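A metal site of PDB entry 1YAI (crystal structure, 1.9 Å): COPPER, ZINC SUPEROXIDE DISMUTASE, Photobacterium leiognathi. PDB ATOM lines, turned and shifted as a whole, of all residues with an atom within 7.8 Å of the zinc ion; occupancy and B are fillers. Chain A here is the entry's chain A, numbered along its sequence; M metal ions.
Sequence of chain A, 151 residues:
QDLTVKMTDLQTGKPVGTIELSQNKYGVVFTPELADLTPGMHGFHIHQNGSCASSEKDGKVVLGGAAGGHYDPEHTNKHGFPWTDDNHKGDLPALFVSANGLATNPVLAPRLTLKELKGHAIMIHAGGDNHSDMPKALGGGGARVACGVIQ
The zinc ion is bound by a ring nitrogen (ND1) of His 70, the side-chain carboxylate of Asp 91, a ring nitrogen (ND1) of His 79 and a ring nitrogen (ND1) of His 88. The zinc ion has four donor atoms within binding distance.
A ring nitrogen (NE2) of His 70 sits close to a ring nitrogen (ND1) of His 45, 3.0 Å away. The backbone NH of His 79 lies within hydrogen-bond range of the side-chain carboxylate of Asp 133. The side-chain carboxylate of Asp 91 sits at hydrogen-bond distance from the backbone NH of Gly 80 (2.9 Å). The backbone NH (N) of His 88 sits at hydrogen-bond distance from the side-chain hydroxyl (OG1) of Thr 76, at 3.1 Å. NE2 of His 79 lies within hydrogen-bond range of OD1 of Asp 129 (2.7 Å). The backbone NH of His 88 is in hydrogen-bond range of the backbone carbonyl oxygen of Lys 78 (2.8 Å). The side-chain carboxylate of Asp 91 sits close to the side-chain amide oxygen of Asn 87.
Of the 26 residues printed, 4 come within 4 Å of the zinc ion.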
ATOM      1  N   PHE A  44      25.765 -17.131 -19.963  1.00  0.00           N
ATOM      2  CA  PHE A  44      26.383 -15.819 -20.135  1.00  0.00           C
ATOM      3  C   PHE A  44      26.017 -14.973 -18.921  1.00  0.00           C
ATOM      4  O   PHE A  44      24.840 -14.630 -18.730  1.00  0.00           O
ATOM      5  CB  PHE A  44      25.739 -15.266 -21.436  1.00  0.00           C
ATOM      6  CG  PHE A  44      26.316 -13.967 -22.000  1.00  0.00           C
ATOM      7  CD1 PHE A  44      27.698 -13.803 -22.073  1.00  0.00           C
ATOM      8  CD2 PHE A  44      25.493 -12.930 -22.436  1.00  0.00           C
ATOM      9  CE1 PHE A  44      28.283 -12.649 -22.591  1.00  0.00           C
ATOM     10  CE2 PHE A  44      26.071 -11.775 -22.999  1.00  0.00           C
ATOM     11  CZ  PHE A  44      27.457 -11.604 -23.022  1.00  0.00           C
ATOM     12  N   HIS A  45      27.027 -14.614 -18.124  1.00  0.00           N
ATOM     13  CA  HIS A  45      26.738 -13.880 -16.902  1.00  0.00           C
ATOM     14  C   HIS A  45      27.810 -12.892 -16.532  1.00  0.00           C
ATOM     15  O   HIS A  45      28.969 -13.021 -16.957  1.00  0.00           O
ATOM     16  CB  HIS A  45      26.671 -14.856 -15.677  1.00  0.00           C
ATOM     17  CG  HIS A  45      26.074 -16.219 -15.931  1.00  0.00           C
ATOM     18  ND1 HIS A  45      26.795 -17.388 -15.811  1.00  0.00           N
ATOM     19  CD2 HIS A  45      24.808 -16.555 -16.346  1.00  0.00           C
ATOM     20  CE1 HIS A  45      25.990 -18.395 -16.102  1.00  0.00           C
ATOM     21  NE2 HIS A  45      24.781 -17.920 -16.452  1.00  0.00           N
ATOM     22  N   ILE A  46      27.424 -11.976 -15.645  1.00  0.00           N
ATOM     23  CA  ILE A  46      28.394 -11.051 -15.119  1.00  0.00           C
ATOM     24  C   ILE A  46      28.822 -11.642 -13.778  1.00  0.00           C
ATOM     25  O   ILE A  46      27.985 -12.004 -12.941  1.00  0.00           O
ATOM     26  CB  ILE A  46      27.776  -9.701 -14.804  1.00  0.00           C
ATOM     27  CG1 ILE A  46      27.157  -9.077 -16.058  1.00  0.00           C
ATOM     28  CG2 ILE A  46      28.857  -8.805 -14.196  1.00  0.00           C
ATOM     29  CD1 ILE A  46      28.196  -8.646 -17.068  1.00  0.00           C
ATOM     30  N   HIS A  47      30.142 -11.779 -13.564  1.00  0.00           N
ATOM     31  CA  HIS A  47      30.678 -12.316 -12.304  1.00  0.00           C
ATOM     32  C   HIS A  47      31.225 -11.206 -11.425  1.00  0.00           C
ATOM     33  O   HIS A  47      31.569 -10.131 -11.914  1.00  0.00           O
ATOM     34  CB  HIS A  47      31.761 -13.364 -12.553  1.00  0.00           C
ATOM     35  CG  HIS A  47      31.187 -14.683 -12.950  1.00  0.00           C
ATOM     36  ND1 HIS A  47      31.489 -15.857 -12.250  1.00  0.00           N
ATOM     37  CD2 HIS A  47      30.328 -14.995 -13.944  1.00  0.00           C
ATOM     38  CE1 HIS A  47      30.813 -16.862 -12.821  1.00  0.00           C
ATOM     39  NE2 HIS A  47      30.113 -16.354 -13.824  1.00  0.00           N
ATOM     40  N   GLY A  69      31.872 -15.751  -8.088  1.00  0.00           N
ATOM     41  CA  GLY A  69      30.527 -16.140  -8.460  1.00  0.00           C
ATOM     42  C   GLY A  69      29.827 -15.045  -9.241  1.00  0.00           C
ATOM     43  O   GLY A  69      30.479 -14.115  -9.706  1.00  0.00           O
ATOM     44  N   HIS A  70      28.505 -15.165  -9.364  1.00  0.00           N
ATOM     45  CA  HIS A  70      27.725 -14.205 -10.116  1.00  0.00           C
ATOM     46  C   HIS A  70      27.590 -12.893  -9.373  1.00  0.00           C
ATOM     47  O   HIS A  70      27.472 -12.907  -8.154  1.00  0.00           O
ATOM     48  CB  HIS A  70      26.311 -14.725 -10.438  1.00  0.00           C
ATOM     49  CG  HIS A  70      26.283 -15.869 -11.388  1.00  0.00           C
ATOM     50  ND1 HIS A  70      25.089 -16.398 -11.831  1.00  0.00           N
ATOM     51  CD2 HIS A  70      27.293 -16.543 -12.010  1.00  0.00           C
ATOM     52  CE1 HIS A  70      25.392 -17.363 -12.683  1.00  0.00           C
ATOM     53  NE2 HIS A  70      26.704 -17.492 -12.793  1.00  0.00           N
ATOM     54  N   TYR A  71      27.595 -11.788 -10.142  1.00  0.00           N
ATOM     55  CA  TYR A  71      27.417 -10.465  -9.637  1.00  0.00           C
ATOM     56  C   TYR A  71      26.089 -10.491  -8.928  1.00  0.00           C
ATOM     57  O   TYR A  71      25.043 -10.773  -9.519  1.00  0.00           O
ATOM     58  CB  TYR A  71      27.400  -9.456 -10.834  1.00  0.00           C
ATOM     59  CG  TYR A  71      27.103  -8.022 -10.461  1.00  0.00           C
ATOM     60  CD1 TYR A  71      27.835  -7.382  -9.447  1.00  0.00           C
ATOM     61  CD2 TYR A  71      26.118  -7.292 -11.129  1.00  0.00           C
ATOM     62  CE1 TYR A  71      27.593  -6.043  -9.144  1.00  0.00           C
ATOM     63  CE2 TYR A  71      25.847  -5.960 -10.817  1.00  0.00           C
ATOM     64  CZ  TYR A  71      26.605  -5.354  -9.830  1.00  0.00           C
ATOM     65  OH  TYR A  71      26.343  -4.058  -9.516  1.00  0.00           O
ATOM     66  N   ASP A  72      26.085 -10.173  -7.622  1.00  0.00           N
ATOM     67  CA  ASP A  72      24.857 -10.245  -6.812  1.00  0.00           C
ATOM     68  C   ASP A  72      24.886  -9.234  -5.665  1.00  0.00           C
ATOM     69  O   ASP A  72      24.946  -9.546  -4.474  1.00  0.00           O
ATOM     70  CB  ASP A  72      24.826 -11.691  -6.266  1.00  0.00           C
ATOM     71  CG  ASP A  72      23.626 -12.032  -5.442  1.00  0.00           C
ATOM     72  OD1 ASP A  72      22.509 -11.404  -5.686  1.00  0.00           O
ATOM     73  OD2 ASP A  72      23.691 -12.896  -4.599  1.00  0.00           O
ATOM     74  N   THR A  76      21.151 -11.954  -3.113  1.00  0.00           N
ATOM     75  CA  THR A  76      20.011 -12.815  -3.299  1.00  0.00           C
ATOM     76  C   THR A  76      20.420 -14.268  -3.087  1.00  0.00           C
ATOM     77  O   THR A  76      19.601 -15.119  -2.739  1.00  0.00           O
ATOM     78  CB  THR A  76      19.405 -12.689  -4.725  1.00  0.00           C
ATOM     79  OG1 THR A  76      20.387 -13.027  -5.710  1.00  0.00           O
ATOM     80  CG2 THR A  76      18.958 -11.238  -4.958  1.00  0.00           C
ATOM     81  N   ASN A  77      21.680 -14.547  -3.413  1.00  0.00           N
ATOM     82  CA  ASN A  77      22.198 -15.905  -3.344  1.00  0.00           C
ATOM     83  C   ASN A  77      21.461 -16.931  -4.173  1.00  0.00           C
ATOM     84  O   ASN A  77      21.427 -18.097  -3.812  1.00  0.00           O
ATOM     85  CB  ASN A  77      22.357 -16.407  -1.918  1.00  0.00           C
ATOM     86  CG  ASN A  77      23.312 -15.498  -1.168  1.00  0.00           C
ATOM     87  OD1 ASN A  77      24.462 -15.317  -1.560  1.00  0.00           O
ATOM     88  ND2 ASN A  77      22.839 -14.954  -0.041  1.00  0.00           N
ATOM     89  N   LYS A  78      20.900 -16.519  -5.304  1.00  0.00           N
ATOM     90  CA  LYS A  78      20.201 -17.429  -6.200  1.00  0.00           C
ATOM     91  C   LYS A  78      20.292 -17.043  -7.646  1.00  0.00           C
ATOM     92  O   LYS A  78      20.265 -15.867  -7.987  1.00  0.00           O
ATOM     93  CB  LYS A  78      18.768 -17.791  -5.832  1.00  0.00           C
ATOM     94  CG  LYS A  78      17.922 -16.677  -5.308  1.00  0.00           C
ATOM     95  CD  LYS A  78      16.708 -17.218  -4.561  1.00  0.00           C
ATOM     96  CE  LYS A  78      15.959 -16.144  -3.776  1.00  0.00           C
ATOM     97  NZ  LYS A  78      16.810 -15.418  -2.807  1.00  0.00           N
ATOM     98  N   HIS A  79      20.370 -18.057  -8.484  1.00  0.00           N
ATOM     99  CA  HIS A  79      20.444 -17.841  -9.920  1.00  0.00           C
ATOM    100  C   HIS A  79      19.034 -17.808 -10.502  1.00  0.00           C
ATOM    101  O   HIS A  79      18.172 -18.538 -10.056  1.00  0.00           O
ATOM    102  CB  HIS A  79      21.259 -19.001 -10.513  1.00  0.00           C
ATOM    103  CG  HIS A  79      21.474 -18.820 -11.991  1.00  0.00           C
ATOM    104  ND1 HIS A  79      22.352 -17.837 -12.455  1.00  0.00           N
ATOM    105  CD2 HIS A  79      20.937 -19.452 -13.073  1.00  0.00           C
ATOM    106  CE1 HIS A  79      22.354 -17.876 -13.792  1.00  0.00           C
ATOM    107  NE2 HIS A  79      21.499 -18.868 -14.198  1.00  0.00           N
ATOM    108  N   GLY A  80      18.784 -16.948 -11.505  1.00  0.00           N
ATOM    109  CA  GLY A  80      17.454 -16.834 -12.094  1.00  0.00           C
ATOM    110  C   GLY A  80      17.435 -16.225 -13.505  1.00  0.00           C
ATOM    111  O   GLY A  80      18.374 -16.429 -14.276  1.00  0.00           O
ATOM    112  N   PHE A  81      16.352 -15.497 -13.835  1.00  0.00           N
ATOM    113  CA  PHE A  81      16.164 -14.869 -15.142  1.00  0.00           C
ATOM    114  C   PHE A  81      16.716 -13.474 -15.139  1.00  0.00           C
ATOM    115  O   PHE A  81      16.901 -12.844 -14.086  1.00  0.00           O
ATOM    116  CB  PHE A  81      14.667 -14.785 -15.496  1.00  0.00           C
ATOM    117  CG  PHE A  81      14.067 -16.140 -15.744  1.00  0.00           C
ATOM    118  CD1 PHE A  81      14.151 -16.728 -16.998  1.00  0.00           C
ATOM    119  CD2 PHE A  81      13.412 -16.839 -14.741  1.00  0.00           C
ATOM    120  CE1 PHE A  81      13.590 -17.963 -17.301  1.00  0.00           C
ATOM    121  CE2 PHE A  81      12.841 -18.089 -15.011  1.00  0.00           C
ATOM    122  CZ  PHE A  81      12.932 -18.651 -16.280  1.00  0.00           C
ATOM    123  N   ASN A  87      17.180 -12.629  -7.784  1.00  0.00           N
ATOM    124  CA  ASN A  87      18.283 -13.487  -8.107  1.00  0.00           C
ATOM    125  C   ASN A  87      19.443 -12.607  -8.550  1.00  0.00           C
ATOM    126  O   ASN A  87      19.292 -11.364  -8.617  1.00  0.00           O
ATOM    127  CB  ASN A  87      17.870 -14.472  -9.232  1.00  0.00           C
ATOM    128  CG  ASN A  87      17.349 -13.798 -10.493  1.00  0.00           C
ATOM    129  OD1 ASN A  87      18.131 -13.552 -11.445  1.00  0.00           O
ATOM    130  ND2 ASN A  87      16.050 -13.439 -10.504  1.00  0.00           N
ATOM    131  N   HIS A  88      20.592 -13.229  -8.827  1.00  0.00           N
ATOM    132  CA  HIS A  88      21.781 -12.491  -9.232  1.00  0.00           C
ATOM    133  C   HIS A  88      21.497 -11.407 -10.303  1.00  0.00           C
ATOM    134  O   HIS A  88      20.996 -11.683 -11.408  1.00  0.00           O
ATOM    135  CB  HIS A  88      22.860 -13.418  -9.814  1.00  0.00           C
ATOM    136  CG  HIS A  88      23.198 -14.618  -8.975  1.00  0.00           C
ATOM    137  ND1 HIS A  88      23.337 -15.881  -9.519  1.00  0.00           N
ATOM    138  CD2 HIS A  88      23.357 -14.720  -7.643  1.00  0.00           C
ATOM    139  CE1 HIS A  88      23.615 -16.717  -8.552  1.00  0.00           C
ATOM    140  NE2 HIS A  88      23.650 -16.045  -7.415  1.00  0.00           N
ATOM    141  N   LYS A  89      21.837 -10.175 -10.014  1.00  0.00           N
ATOM    142  CA  LYS A  89      21.677  -9.148 -11.011  1.00  0.00           C
ATOM    143  C   LYS A  89      22.607  -9.435 -12.222  1.00  0.00           C
ATOM    144  O   LYS A  89      22.375  -8.895 -13.314  1.00  0.00           O
ATOM    145  CB  LYS A  89      22.115  -7.834 -10.392  1.00  0.00           C
ATOM    146  CG  LYS A  89      21.317  -6.628 -10.794  1.00  0.00           C
ATOM    147  CD  LYS A  89      21.693  -5.416  -9.972  1.00  0.00           C
ATOM    148  CE  LYS A  89      20.804  -4.249 -10.282  1.00  0.00           C
ATOM    149  NZ  LYS A  89      21.301  -3.050  -9.625  1.00  0.00           N
ATOM    150  N   GLY A  90      23.675 -10.241 -12.053  1.00  0.00           N
ATOM    151  CA  GLY A  90      24.557 -10.539 -13.166  1.00  0.00           C
ATOM    152  C   GLY A  90      23.997 -11.591 -14.141  1.00  0.00           C
ATOM    153  O   GLY A  90      24.685 -12.003 -15.047  1.00  0.00           O
ATOM    154  N   ASP A  91      22.733 -12.042 -13.983  1.00  0.00           N
ATOM    155  CA  ASP A  91      22.157 -13.053 -14.837  1.00  0.00           C
ATOM    156  C   ASP A  91      21.681 -12.500 -16.175  1.00  0.00           C
ATOM    157  O   ASP A  91      20.647 -11.854 -16.197  1.00  0.00           O
ATOM    158  CB  ASP A  91      21.037 -13.865 -14.105  1.00  0.00           C
ATOM    159  CG  ASP A  91      21.617 -14.642 -12.919  1.00  0.00           C
ATOM    160  OD1 ASP A  91      22.784 -14.998 -12.851  1.00  0.00           O
ATOM    161  OD2 ASP A  91      20.723 -14.861 -11.989  1.00  0.00           O
ATOM    162  N   LEU A  92      22.432 -12.786 -17.262  1.00  0.00           N
ATOM    163  CA  LEU A  92      22.094 -12.303 -18.573  1.00  0.00           C
ATOM    164  C   LEU A  92      21.383 -13.390 -19.370  1.00  0.00           C
ATOM    165  O   LEU A  92      21.494 -14.554 -19.047  1.00  0.00           O
ATOM    166  CB  LEU A  92      23.398 -11.918 -19.313  1.00  0.00           C
ATOM    167  CG  LEU A  92      24.378 -11.090 -18.482  1.00  0.00           C
ATOM    168  CD1 LEU A  92      25.621 -10.888 -19.320  1.00  0.00           C
ATOM    169  CD2 LEU A  92      23.809  -9.719 -18.071  1.00  0.00           C
ATOM    170  N   ASP A 129      22.043 -22.301 -19.999  1.00  0.00           N
ATOM    171  CA  ASP A 129      21.504 -21.637 -18.846  1.00  0.00           C
ATOM    172  C   ASP A 129      19.993 -21.744 -18.870  1.00  0.00           C
ATOM    173  O   ASP A 129      19.400 -21.137 -19.717  1.00  0.00           O
ATOM    174  CB  ASP A 129      21.839 -20.134 -18.866  1.00  0.00           C
ATOM    175  CG  ASP A 129      21.663 -19.446 -17.536  1.00  0.00           C
ATOM    176  OD1 ASP A 129      21.051 -19.941 -16.633  1.00  0.00           O
ATOM    177  OD2 ASP A 129      22.326 -18.315 -17.410  1.00  0.00           O
ATOM    178  N   HIS A 131      18.301 -20.665 -16.351  1.00  0.00           N
ATOM    179  CA  HIS A 131      17.907 -19.621 -15.411  1.00  0.00           C
ATOM    180  C   HIS A 131      17.345 -20.156 -14.109  1.00  0.00           C
ATOM    181  O   HIS A 131      16.388 -19.622 -13.588  1.00  0.00           O
ATOM    182  CB  HIS A 131      16.875 -18.654 -16.041  1.00  0.00           C
ATOM    183  CG  HIS A 131      17.451 -17.980 -17.271  1.00  0.00           C
ATOM    184  ND1 HIS A 131      18.510 -17.076 -17.149  1.00  0.00           N
ATOM    185  CD2 HIS A 131      17.168 -18.144 -18.582  1.00  0.00           C
ATOM    186  CE1 HIS A 131      18.825 -16.700 -18.386  1.00  0.00           C
ATOM    187  NE2 HIS A 131      18.037 -17.332 -19.278  1.00  0.00           N
ATOM    188  N   SER A 132      17.936 -21.189 -13.571  1.00  0.00           N
ATOM    189  CA  SER A 132      17.462 -21.714 -12.337  1.00  0.00           C
ATOM    190  C   SER A 132      18.614 -22.461 -11.701  1.00  0.00           C
ATOM    191  O   SER A 132      19.569 -22.811 -12.382  1.00  0.00           O
ATOM    192  CB  SER A 132      16.368 -22.737 -12.596  1.00  0.00           C
ATOM    193  OG  SER A 132      16.053 -23.273 -11.352  1.00  0.00           O
ATOM    194  N   ASP A 133      18.499 -22.723 -10.400  1.00  0.00           N
ATOM    195  CA  ASP A 133      19.477 -23.532  -9.695  1.00  0.00           C
ATOM    196  C   ASP A 133      19.025 -25.021  -9.702  1.00  0.00           C
ATOM    197  O   ASP A 133      19.688 -25.874  -9.170  1.00  0.00           O
ATOM    198  CB  ASP A 133      19.667 -23.052  -8.265  1.00  0.00           C
ATOM    199  CG  ASP A 133      20.397 -21.763  -8.175  1.00  0.00           C
ATOM    200  OD1 ASP A 133      21.583 -21.821  -8.685  1.00  0.00           O
ATOM    201  OD2 ASP A 133      19.948 -20.792  -7.567  1.00  0.00           O
ATOM    202  N   LEU A 138      23.388 -22.766 -10.654  1.00  0.00           N
ATOM    203  CA  LEU A 138      23.763 -21.745 -11.598  1.00  0.00           C
ATOM    204  C   LEU A 138      23.356 -21.973 -13.053  1.00  0.00           C
ATOM    205  O   LEU A 138      24.090 -21.594 -13.969  1.00  0.00           O
ATOM    206  CB  LEU A 138      25.247 -21.381 -11.475  1.00  0.00           C
ATOM    207  CG  LEU A 138      25.621 -21.271 -10.003  1.00  0.00           C
ATOM    208  CD1 LEU A 138      27.167 -21.338  -9.793  1.00  0.00           C
ATOM    209  CD2 LEU A 138      25.050 -19.974  -9.425  1.00  0.00           C
ATOM    210  N   GLY A 139      22.218 -22.607 -13.285  1.00  0.00           N
ATOM    211  CA  GLY A 139      21.706 -22.827 -14.632  1.00  0.00           C
ATOM    212  C   GLY A 139      22.346 -23.889 -15.472  1.00  0.00           C
ATOM    213  O   GLY A 139      21.967 -24.046 -16.631  1.00  0.00           O
HETATM  214 ZN    ZN M   1      23.323 -16.229 -11.579  1.00  0.00          ZN
HETATM  215 CU    CU M   2      28.551 -17.499 -14.856  1.00  0.00          CU
